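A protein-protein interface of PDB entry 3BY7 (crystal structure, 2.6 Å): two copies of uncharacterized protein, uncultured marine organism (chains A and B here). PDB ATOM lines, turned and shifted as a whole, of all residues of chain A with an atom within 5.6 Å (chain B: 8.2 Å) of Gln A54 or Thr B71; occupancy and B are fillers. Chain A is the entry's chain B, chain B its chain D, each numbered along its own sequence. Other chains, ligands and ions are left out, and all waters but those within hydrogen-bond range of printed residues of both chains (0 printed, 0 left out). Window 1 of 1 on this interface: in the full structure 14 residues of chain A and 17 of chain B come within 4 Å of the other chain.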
ATOM      1  N   ALA A  32     -20.091 -18.582 -10.288  1.00  0.00           N
ATOM      2  CA  ALA A  32     -18.618 -18.489 -10.427  1.00  0.00           C
ATOM      3  C   ALA A  32     -17.904 -19.785 -10.066  1.00  0.00           C
ATOM      4  O   ALA A  32     -18.131 -20.335  -8.997  1.00  0.00           O
ATOM      5  CB  ALA A  32     -18.074 -17.376  -9.555  1.00  0.00           C
ATOM      6  N   PRO A  52     -16.794 -24.720  -7.402  1.00  0.00           N
ATOM      7  CA  PRO A  52     -17.393 -23.453  -6.975  1.00  0.00           C
ATOM      8  C   PRO A  52     -16.391 -22.551  -6.291  1.00  0.00           C
ATOM      9  O   PRO A  52     -15.626 -23.005  -5.448  1.00  0.00           O
ATOM     10  CB  PRO A  52     -18.489 -23.893  -6.005  1.00  0.00           C
ATOM     11  CG  PRO A  52     -18.860 -25.264  -6.457  1.00  0.00           C
ATOM     12  CD  PRO A  52     -17.558 -25.877  -6.899  1.00  0.00           C
ATOM     13  N   TRP A  53     -16.390 -21.280  -6.672  1.00  0.00           N
ATOM     14  CA  TRP A  53     -15.351 -20.361  -6.236  1.00  0.00           C
ATOM     15  C   TRP A  53     -15.472 -20.019  -4.757  1.00  0.00           C
ATOM     16  O   TRP A  53     -14.491 -20.034  -4.032  1.00  0.00           O
ATOM     17  CB  TRP A  53     -15.352 -19.106  -7.107  1.00  0.00           C
ATOM     18  CG  TRP A  53     -14.359 -18.071  -6.681  1.00  0.00           C
ATOM     19  CD1 TRP A  53     -13.089 -18.283  -6.228  1.00  0.00           C
ATOM     20  CD2 TRP A  53     -14.545 -16.661  -6.698  1.00  0.00           C
ATOM     21  NE1 TRP A  53     -12.484 -17.090  -5.946  1.00  0.00           N
ATOM     22  CE2 TRP A  53     -13.363 -16.077  -6.221  1.00  0.00           C
ATOM     23  CE3 TRP A  53     -15.605 -15.832  -7.056  1.00  0.00           C
ATOM     24  CZ2 TRP A  53     -13.212 -14.709  -6.093  1.00  0.00           C
ATOM     25  CZ3 TRP A  53     -15.445 -14.464  -6.932  1.00  0.00           C
ATOM     26  CH2 TRP A  53     -14.261 -13.920  -6.453  1.00  0.00           C
ATOM     27  N   GLN A  54     -16.684 -19.724  -4.318  1.00  0.00           N
ATOM     28  CA  GLN A  54     -16.932 -19.321  -2.949  1.00  0.00           C
ATOM     29  C   GLN A  54     -17.840 -20.378  -2.341  1.00  0.00           C
ATOM     30  O   GLN A  54     -19.063 -20.249  -2.376  1.00  0.00           O
ATOM     31  CB  GLN A  54     -17.597 -17.937  -2.929  1.00  0.00           C
ATOM     32  CG  GLN A  54     -16.745 -16.787  -3.506  1.00  0.00           C
ATOM     33  CD  GLN A  54     -15.751 -16.202  -2.514  1.00  0.00           C
ATOM     34  OE1 GLN A  54     -15.793 -16.497  -1.311  1.00  0.00           O
ATOM     35  NE2 GLN A  54     -14.848 -15.357  -3.017  1.00  0.00           N
ATOM     36  N   PRO A  55     -17.249 -21.457  -1.809  1.00  0.00           N
ATOM     37  CA  PRO A  55     -18.056 -22.546  -1.271  1.00  0.00           C
ATOM     38  C   PRO A  55     -18.678 -22.248   0.093  1.00  0.00           C
ATOM     39  O   PRO A  55     -19.561 -22.988   0.524  1.00  0.00           O
ATOM     40  CB  PRO A  55     -17.059 -23.692  -1.166  1.00  0.00           C
ATOM     41  CG  PRO A  55     -15.787 -23.029  -0.899  1.00  0.00           C
ATOM     42  CD  PRO A  55     -15.811 -21.740  -1.678  1.00  0.00           C
ATOM     43  N   TYR A  56     -18.243 -21.181   0.760  1.00  0.00           N
ATOM     44  CA  TYR A  56     -18.784 -20.860   2.076  1.00  0.00           C
ATOM     45  C   TYR A  56     -20.045 -19.980   2.035  1.00  0.00           C
ATOM     46  O   TYR A  56     -20.492 -19.512   3.072  1.00  0.00           O
ATOM     47  CB  TYR A  56     -17.709 -20.219   2.951  1.00  0.00           C
ATOM     48  CG  TYR A  56     -16.413 -20.997   3.036  1.00  0.00           C
ATOM     49  CD1 TYR A  56     -16.388 -22.386   2.960  1.00  0.00           C
ATOM     50  CD2 TYR A  56     -15.206 -20.333   3.219  1.00  0.00           C
ATOM     51  CE1 TYR A  56     -15.194 -23.083   3.040  1.00  0.00           C
ATOM     52  CE2 TYR A  56     -14.007 -21.022   3.302  1.00  0.00           C
ATOM     53  CZ  TYR A  56     -14.006 -22.394   3.211  1.00  0.00           C
ATOM     54  OH  TYR A  56     -12.810 -23.073   3.299  1.00  0.00           O
ATOM     55  N   THR A  57     -20.631 -19.778   0.856  1.00  0.00           N
ATOM     56  CA  THR A  57     -21.777 -18.876   0.709  1.00  0.00           C
ATOM     57  C   THR A  57     -22.816 -19.405  -0.274  1.00  0.00           C
ATOM     58  O   THR A  57     -22.483 -20.122  -1.206  1.00  0.00           O
ATOM     59  CB  THR A  57     -21.333 -17.497   0.195  1.00  0.00           C
ATOM     60  OG1 THR A  57     -22.450 -16.606   0.180  1.00  0.00           O
ATOM     61  CG2 THR A  57     -20.780 -17.607  -1.210  1.00  0.00           C
ATOM     62  N   ILE A  62     -21.842 -12.239  -6.792  1.00  0.00           N
ATOM     63  CA  ILE A  62     -20.658 -11.819  -6.053  1.00  0.00           C
ATOM     64  C   ILE A  62     -20.047 -10.596  -6.718  1.00  0.00           C
ATOM     65  O   ILE A  62     -19.815 -10.602  -7.928  1.00  0.00           O
ATOM     66  CB  ILE A  62     -19.579 -12.899  -6.091  1.00  0.00           C
ATOM     67  CG1 ILE A  62     -20.112 -14.188  -5.477  1.00  0.00           C
ATOM     68  CG2 ILE A  62     -18.324 -12.430  -5.358  1.00  0.00           C
ATOM     69  CD1 ILE A  62     -19.125 -15.310  -5.491  1.00  0.00           C
ATOM     70  N   VAL A  63     -19.743  -9.575  -5.922  1.00  0.00           N
ATOM     71  CA  VAL A  63     -19.189  -8.340  -6.437  1.00  0.00           C
ATOM     72  C   VAL A  63     -17.702  -8.251  -6.093  1.00  0.00           C
ATOM     73  O   VAL A  63     -17.320  -8.465  -4.940  1.00  0.00           O
ATOM     74  CB  VAL A  63     -19.927  -7.118  -5.835  1.00  0.00           C
ATOM     75  CG1 VAL A  63     -19.345  -5.817  -6.360  1.00  0.00           C
ATOM     76  CG2 VAL A  63     -21.409  -7.192  -6.132  1.00  0.00           C
ATOM     77  N   ILE A  64     -16.881  -7.945  -7.106  1.00  0.00           N
ATOM     78  CA  ILE A  64     -15.474  -7.640  -6.923  1.00  0.00           C
ATOM     79  C   ILE A  64     -15.127  -6.329  -7.613  1.00  0.00           C
ATOM     80  O   ILE A  64     -15.633  -6.045  -8.688  1.00  0.00           O
ATOM     81  CB  ILE A  64     -14.567  -8.744  -7.471  1.00  0.00           C
ATOM     82  CG1 ILE A  64     -15.002  -9.179  -8.878  1.00  0.00           C
ATOM     83  CG2 ILE A  64     -14.615  -9.921  -6.551  1.00  0.00           C
ATOM     84  CD1 ILE A  64     -13.962 -10.057  -9.597  1.00  0.00           C
ATOM     85  N   LYS B   6     -20.427 -11.853   8.030  1.00  0.00           N
ATOM     86  CA  LYS B   6     -20.084 -12.024   6.602  1.00  0.00           C
ATOM     87  C   LYS B   6     -18.722 -12.699   6.458  1.00  0.00           C
ATOM     88  O   LYS B   6     -17.963 -12.795   7.429  1.00  0.00           O
ATOM     89  CB  LYS B   6     -20.016 -10.673   5.898  1.00  0.00           C
ATOM     90  CG  LYS B   6     -21.308  -9.906   5.862  1.00  0.00           C
ATOM     91  CD  LYS B   6     -22.290 -10.475   4.859  1.00  0.00           C
ATOM     92  CE  LYS B   6     -23.229  -9.372   4.390  1.00  0.00           C
ATOM     93  NZ  LYS B   6     -24.527  -9.920   3.936  1.00  0.00           N
ATOM     94  N   ILE B   7     -18.415 -13.161   5.254  1.00  0.00           N
ATOM     95  CA  ILE B   7     -17.118 -13.774   4.969  1.00  0.00           C
ATOM     96  C   ILE B   7     -16.341 -12.876   4.018  1.00  0.00           C
ATOM     97  O   ILE B   7     -16.814 -12.585   2.918  1.00  0.00           O
ATOM     98  CB  ILE B   7     -17.276 -15.203   4.372  1.00  0.00           C
ATOM     99  CG1 ILE B   7     -17.570 -16.189   5.500  1.00  0.00           C
ATOM    100  CG2 ILE B   7     -16.024 -15.648   3.621  1.00  0.00           C
ATOM    101  CD1 ILE B   7     -17.890 -17.601   5.040  1.00  0.00           C
ATOM    102  N   MET B   8     -15.153 -12.448   4.443  1.00  0.00           N
ATOM    103  CA  MET B   8     -14.276 -11.635   3.615  1.00  0.00           C
ATOM    104  C   MET B   8     -13.136 -12.488   3.077  1.00  0.00           C
ATOM    105  O   MET B   8     -12.403 -13.092   3.853  1.00  0.00           O
ATOM    106  CB  MET B   8     -13.639 -10.505   4.447  1.00  0.00           C
ATOM    107  CG  MET B   8     -14.578  -9.441   5.021  1.00  0.00           C
ATOM    108  SD  MET B   8     -13.677  -8.322   6.427  1.00  0.00           S
ATOM    109  CE  MET B   8     -14.046  -9.535   8.009  1.00  0.00           C
ATOM    110  N   ARG B   9     -12.979 -12.530   1.754  1.00  0.00           N
ATOM    111  CA  ARG B   9     -11.772 -13.074   1.135  1.00  0.00           C
ATOM    112  C   ARG B   9     -10.771 -11.946   1.146  1.00  0.00           C
ATOM    113  O   ARG B   9     -11.013 -10.930   0.507  1.00  0.00           O
ATOM    114  CB  ARG B   9     -12.066 -13.509  -0.310  1.00  0.00           C
ATOM    115  CG  ARG B   9     -10.866 -14.095  -1.071  1.00  0.00           C
ATOM    116  CD  ARG B   9     -10.461 -15.502  -0.591  1.00  0.00           C
ATOM    117  NE  ARG B   9     -11.460 -16.520  -0.950  1.00  0.00           N
ATOM    118  CZ  ARG B   9     -11.446 -17.267  -2.059  1.00  0.00           C
ATOM    119  NH1 ARG B   9     -10.482 -17.142  -2.983  1.00  0.00           N
ATOM    120  NH2 ARG B   9     -12.429 -18.146  -2.254  1.00  0.00           N
ATOM    121  N   LEU B  10      -9.667 -12.097   1.870  1.00  0.00           N
ATOM    122  CA  LEU B  10      -8.636 -11.074   1.847  1.00  0.00           C
ATOM    123  C   LEU B  10      -7.734 -11.197   0.612  1.00  0.00           C
ATOM    124  O   LEU B  10      -7.766 -12.164  -0.149  1.00  0.00           O
ATOM    125  CB  LEU B  10      -7.824 -11.073   3.128  1.00  0.00           C
ATOM    126  CG  LEU B  10      -8.714 -10.934   4.371  1.00  0.00           C
ATOM    127  CD1 LEU B  10      -7.894 -10.577   5.582  1.00  0.00           C
ATOM    128  CD2 LEU B  10      -9.828  -9.897   4.200  1.00  0.00           C
ATOM    129  N   VAL B  11      -6.961 -10.147   0.409  1.00  0.00           N
ATOM    130  CA  VAL B  11      -6.074 -10.039  -0.728  1.00  0.00           C
ATOM    131  C   VAL B  11      -4.857 -10.945  -0.485  1.00  0.00           C
ATOM    132  O   VAL B  11      -4.199 -11.367  -1.427  1.00  0.00           O
ATOM    133  CB  VAL B  11      -5.739  -8.529  -0.988  1.00  0.00           C
ATOM    134  CG1 VAL B  11      -4.544  -8.049  -0.180  1.00  0.00           C
ATOM    135  CG2 VAL B  11      -5.539  -8.309  -2.428  1.00  0.00           C
ATOM    136  N   GLU B  14      -6.658 -15.393   2.503  1.00  0.00           N
ATOM    137  CA  GLU B  14      -7.423 -16.010   3.592  1.00  0.00           C
ATOM    138  C   GLU B  14      -8.918 -15.740   3.469  1.00  0.00           C
ATOM    139  O   GLU B  14      -9.330 -14.812   2.778  1.00  0.00           O
ATOM    140  CB  GLU B  14      -6.981 -15.488   4.965  1.00  0.00           C
ATOM    141  CG  GLU B  14      -5.476 -15.314   5.177  1.00  0.00           C
ATOM    142  CD  GLU B  14      -5.183 -14.109   6.067  1.00  0.00           C
ATOM    143  OE1 GLU B  14      -5.548 -14.149   7.277  1.00  0.00           O
ATOM    144  OE2 GLU B  14      -4.602 -13.121   5.542  1.00  0.00           O
ATOM    145  N   ASP B  15      -9.714 -16.565   4.140  1.00  0.00           N
ATOM    146  CA  ASP B  15     -11.142 -16.330   4.307  1.00  0.00           C
ATOM    147  C   ASP B  15     -11.436 -16.019   5.767  1.00  0.00           C
ATOM    148  O   ASP B  15     -11.168 -16.837   6.631  1.00  0.00           O
ATOM    149  CB  ASP B  15     -11.942 -17.559   3.876  1.00  0.00           C
ATOM    150  CG  ASP B  15     -11.999 -17.718   2.366  1.00  0.00           C
ATOM    151  OD1 ASP B  15     -12.471 -16.768   1.698  1.00  0.00           O
ATOM    152  OD2 ASP B  15     -11.580 -18.784   1.838  1.00  0.00           O
ATOM    153  N   ILE B  16     -11.971 -14.836   6.038  1.00  0.00           N
ATOM    154  CA  ILE B  16     -12.249 -14.385   7.404  1.00  0.00           C
ATOM    155  C   ILE B  16     -13.761 -14.313   7.634  1.00  0.00           C
ATOM    156  O   ILE B  16     -14.524 -13.955   6.730  1.00  0.00           O
ATOM    157  CB  ILE B  16     -11.644 -12.974   7.673  1.00  0.00           C
ATOM    158  CG1 ILE B  16     -10.126 -12.997   7.541  1.00  0.00           C
ATOM    159  CG2 ILE B  16     -11.969 -12.500   9.046  1.00  0.00           C
ATOM    160  CD1 ILE B  16      -9.463 -14.023   8.378  1.00  0.00           C
ATOM    161  N   ILE B  27     -13.547  -1.195   6.988  1.00  0.00           N
ATOM    162  CA  ILE B  27     -14.353  -2.268   7.521  1.00  0.00           C
ATOM    163  C   ILE B  27     -13.878  -2.520   8.935  1.00  0.00           C
ATOM    164  O   ILE B  27     -12.684  -2.733   9.155  1.00  0.00           O
ATOM    165  CB  ILE B  27     -14.158  -3.575   6.731  1.00  0.00           C
ATOM    166  CG1 ILE B  27     -14.528  -3.397   5.260  1.00  0.00           C
ATOM    167  CG2 ILE B  27     -14.974  -4.698   7.347  1.00  0.00           C
ATOM    168  CD1 ILE B  27     -14.380  -4.675   4.472  1.00  0.00           C
ATOM    169  N   ASP B  66     -10.991  -1.382   2.768  1.00  0.00           N
ATOM    170  CA  ASP B  66     -11.780  -2.223   1.889  1.00  0.00           C
ATOM    171  C   ASP B  66     -10.996  -2.617   0.632  1.00  0.00           C
ATOM    172  O   ASP B  66     -11.347  -3.574  -0.050  1.00  0.00           O
ATOM    173  CB  ASP B  66     -13.079  -1.491   1.491  1.00  0.00           C
ATOM    174  CG  ASP B  66     -12.827  -0.283   0.571  1.00  0.00           C
ATOM    175  OD1 ASP B  66     -12.496   0.822   1.069  1.00  0.00           O
ATOM    176  OD2 ASP B  66     -12.966  -0.428  -0.663  1.00  0.00           O
ATOM    177  N   LYS B  68      -8.240  -4.046   0.683  1.00  0.00           N
ATOM    178  CA  LYS B  68      -7.562  -5.301   0.997  1.00  0.00           C
ATOM    179  C   LYS B  68      -8.518  -6.489   1.013  1.00  0.00           C
ATOM    180  O   LYS B  68      -8.124  -7.575   1.415  1.00  0.00           O
ATOM    181  CB  LYS B  68      -6.835  -5.234   2.348  1.00  0.00           C
ATOM    182  CG  LYS B  68      -5.966  -3.987   2.610  1.00  0.00           C
ATOM    183  CD  LYS B  68      -4.755  -3.891   1.701  1.00  0.00           C
ATOM    184  CE  LYS B  68      -4.386  -2.419   1.393  1.00  0.00           C
ATOM    185  N   VAL B  69      -9.765  -6.281   0.584  1.00  0.00           N
ATOM    186  CA  VAL B  69     -10.779  -7.343   0.538  1.00  0.00           C
ATOM    187  C   VAL B  69     -11.239  -7.583  -0.899  1.00  0.00           C
ATOM    188  O   VAL B  69     -11.612  -6.645  -1.584  1.00  0.00           O
ATOM    189  CB  VAL B  69     -12.002  -6.976   1.399  1.00  0.00           C
ATOM    190  CG1 VAL B  69     -13.090  -8.009   1.224  1.00  0.00           C
ATOM    191  CG2 VAL B  69     -11.605  -6.863   2.878  1.00  0.00           C
ATOM    192  N   ILE B  70     -11.212  -8.836  -1.345  1.00  0.00           N
ATOM    193  CA  ILE B  70     -11.634  -9.171  -2.705  1.00  0.00           C
ATOM    194  C   ILE B  70     -13.158  -9.370  -2.817  1.00  0.00           C
ATOM    195  O   ILE B  70     -13.781  -8.855  -3.748  1.00  0.00           O
ATOM    196  CB  ILE B  70     -10.869 -10.399  -3.270  1.00  0.00           C
ATOM    197  CG1 ILE B  70      -9.374 -10.122  -3.280  1.00  0.00           C
ATOM    198  CG2 ILE B  70     -11.284 -10.705  -4.716  1.00  0.00           C
ATOM    199  CD1 ILE B  70      -8.556 -11.346  -3.313  1.00  0.00           C
ATOM    200  N   THR B  71     -13.750 -10.116  -1.888  1.00  0.00           N
ATOM    201  CA  THR B  71     -15.205 -10.320  -1.869  1.00  0.00           C
ATOM    202  C   THR B  71     -15.710 -10.246  -0.445  1.00  0.00           C
ATOM    203  O   THR B  71     -14.983 -10.582   0.490  1.00  0.00           O
ATOM    204  CB  THR B  71     -15.613 -11.691  -2.457  1.00  0.00           C
ATOM    205  OG1 THR B  71     -14.763 -12.715  -1.937  1.00  0.00           O
ATOM    206  CG2 THR B  71     -15.506 -11.710  -3.974  1.00  0.00           C
ATOM    207  N   ILE B  72     -16.943  -9.781  -0.279  1.00  0.00           N
ATOM    208  CA  ILE B  72     -17.651  -9.889   0.996  1.00  0.00           C
ATOM    209  C   ILE B  72     -18.957 -10.605   0.716  1.00  0.00           C
ATOM    210  O   ILE B  72     -19.711 -10.225  -0.165  1.00  0.00           O
ATOM    211  CB  ILE B  72     -17.894  -8.542   1.669  1.00  0.00           C
ATOM    212  CG1 ILE B  72     -16.566  -7.834   1.931  1.00  0.00           C
ATOM    213  CG2 ILE B  72     -18.600  -8.750   2.990  1.00  0.00           C
ATOM    214  CD1 ILE B  72     -16.707  -6.427   2.450  1.00  0.00           C
ATOM    215  N   THR B  73     -19.221 -11.650   1.483  1.00  0.00           N
ATOM    216  CA  THR B  73     -20.167 -12.665   1.084  1.00  0.00           C
ATOM    217  C   THR B  73     -20.846 -13.212   2.342  1.00  0.00           C
ATOM    218  O   THR B  73     -20.221 -13.290   3.396  1.00  0.00           O
ATOM    219  CB  THR B  73     -19.396 -13.751   0.286  1.00  0.00           C
ATOM    220  OG1 THR B  73     -20.306 -14.559  -0.450  1.00  0.00           O
ATOM    221  CG2 THR B  73     -18.543 -14.630   1.202  1.00  0.00           C
ATOM    222  N   SER B  74     -22.133 -13.542   2.247  1.00  0.00           N
ATOM    223  CA  SER B  74     -22.880 -14.033   3.403  1.00  0.00           C
ATOM    224  C   SER B  74     -22.823 -15.569   3.494  1.00  0.00           C
ATOM    225  O   SER B  74     -23.134 -16.267   2.537  1.00  0.00           O
ATOM    226  CB  SER B  74     -24.324 -13.539   3.356  1.00  0.00           C
ATOM    227  OG  SER B  74     -24.899 -13.771   2.085  1.00  0.00           O
ATOM    228  N   LYS B  76     -23.035 -19.705   4.414  1.00  0.00           N
ATOM    229  CA  LYS B  76     -24.019 -20.790   4.497  1.00  0.00           C
ATOM    230  C   LYS B  76     -24.450 -21.010   5.950  1.00  0.00           C
ATOM    231  O   LYS B  76     -23.676 -20.773   6.881  1.00  0.00           O
ATOM    232  CB  LYS B  76     -23.440 -22.094   3.918  1.00  0.00           C
ATOM    233  CG  LYS B  76     -23.237 -22.091   2.408  1.00  0.00           C
ATOM    234  CD  LYS B  76     -22.853 -23.480   1.883  1.00  0.00           C
ATOM    235  CE  LYS B  76     -22.530 -23.479   0.371  1.00  0.00           C
ATOM    236  N   ILE B  79     -22.244 -22.704   8.502  1.00  0.00           N
ATOM    237  CA  ILE B  79     -21.086 -21.928   8.938  1.00  0.00           C
ATOM    238  C   ILE B  79     -21.443 -20.845   9.964  1.00  0.00           C
ATOM    239  O   ILE B  79     -20.653 -20.561  10.867  1.00  0.00           O
ATOM    240  CB  ILE B  79     -20.374 -21.304   7.742  1.00  0.00           C
ATOM    241  CG1 ILE B  79     -19.933 -22.416   6.774  1.00  0.00           C
ATOM    242  CG2 ILE B  79     -19.189 -20.489   8.217  1.00  0.00           C
ATOM    243  CD1 ILE B  79     -19.136 -21.950   5.610  1.00  0.00           C
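The side-chain hydroxyl (OG1) of Thr B71 sits at hydrogen-bond distance from the side-chain amide nitrogen (NE2) of Gln A54 (2.9 Å).
The side-chain hydroxyl (OG1) of Thr A57 sits at hydrogen-bond distance from the side-chain hydroxyl (OG1) of Thr B73, at 3.0 Å.
The backbone carbonyl oxygen (O) of Trp A53 sits at hydrogen-bond distance from the guanidinium group (NH2) of Arg B9, 3.3 Å away.
O of Tyr A56 is in hydrogen-bond range of N of Lys B76 (2.9 Å).
OG1 of Thr A57 sits at hydrogen-bond distance from O of Ser B74, 2.5 Å away.
N of Trp A53 sits at hydrogen-bond distance from O of Ala A32.
N of Ile B7 is in hydrogen-bond range of O of Thr B73, 2.6 Å away.
The backbone carbonyl oxygen of Arg B9 is in hydrogen-bond range of the backbone NH of Ile B70 (2.8 Å).
The backbone carbonyl oxygen of Thr B71 lies within hydrogen-bond range of the backbone NH of Arg B9 (3.1 Å).
The side-chain carboxylate (OD1) of Asp B15 lies within salt-bridge range of the guanidinium group (NE) of Arg B9 (2.8 Å).
Trp A53 touches Thr B71 (CH2 to CG2, 3.5 Å).
Arg B9 touches Gln A54.
Ile B7 touches Tyr A56 (CD1 to CB, 3.4 Å).
CE2 of Tyr A56 touches OD2 of Asp B15, 3.6 Å away.
Tyr A56 touches Ile B79 (CB to CD1, 3.5 Å).
Thr B71 touches Ile A62 (CG2 to CG2, 3.2 Å).
Ile B70 touches Val A63.
Val A63 touches Thr B71.
Ile B70 touches Ile A64 (O to CG2, 3.1 Å).
CG2 of Thr B71 touches CG2 of Ile A64, at 3.3 Å.
Gln A54 touches two residues of chain B.
Of chain B, only Lys B76 comes within 4 Å of Pro A55.
Of the printed residues of chain B, Tyr A56 touches Ile B7, Asp B15, Lys B76 and Ile B79.
Of the printed residues of chain B, Thr A57 touches Thr B73 (3.0 Å), Ser B74 (2.5 Å) and Lys B76 (3.7 Å).
Printed residues of chain B within 4 Å of Val A63: Ile B70 (3.8 Å) and Thr B71 (3.8 Å).
Of the printed residues of chain A, Ile B7 touches Tyr A56 (3.4 Å).
Printed residues of chain A within 4 Å of Arg B9: Trp A53 and Gln A54.
Thr B71 touches five residues of chain A.
The nearest residue of chain B that does not touch Gln A54 is Thr B73 (4.2 Å).
The nearest printed residue of chain A that does not touch Thr B71 is Thr A57 (7.8 Å).
Printed residues of chain A that touch a printed residue of chain B: Trp A53, Gln A54, Pro A55, Tyr A56, Thr A57, Ile A62, Val A63 and Ile A64.
Of the 20 printed residues of chain B, 9 touch a printed residue of chain A.
Among the printed residues, no Asp or Glu carboxylate lies within 4 Å of a Lys or Arg side-chain nitrogen of the other chain.
No position is printed for both chains.
Of the 17 pairs that touch across the chains among the printed residues, none has its exchanged pair printed and touching as well.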
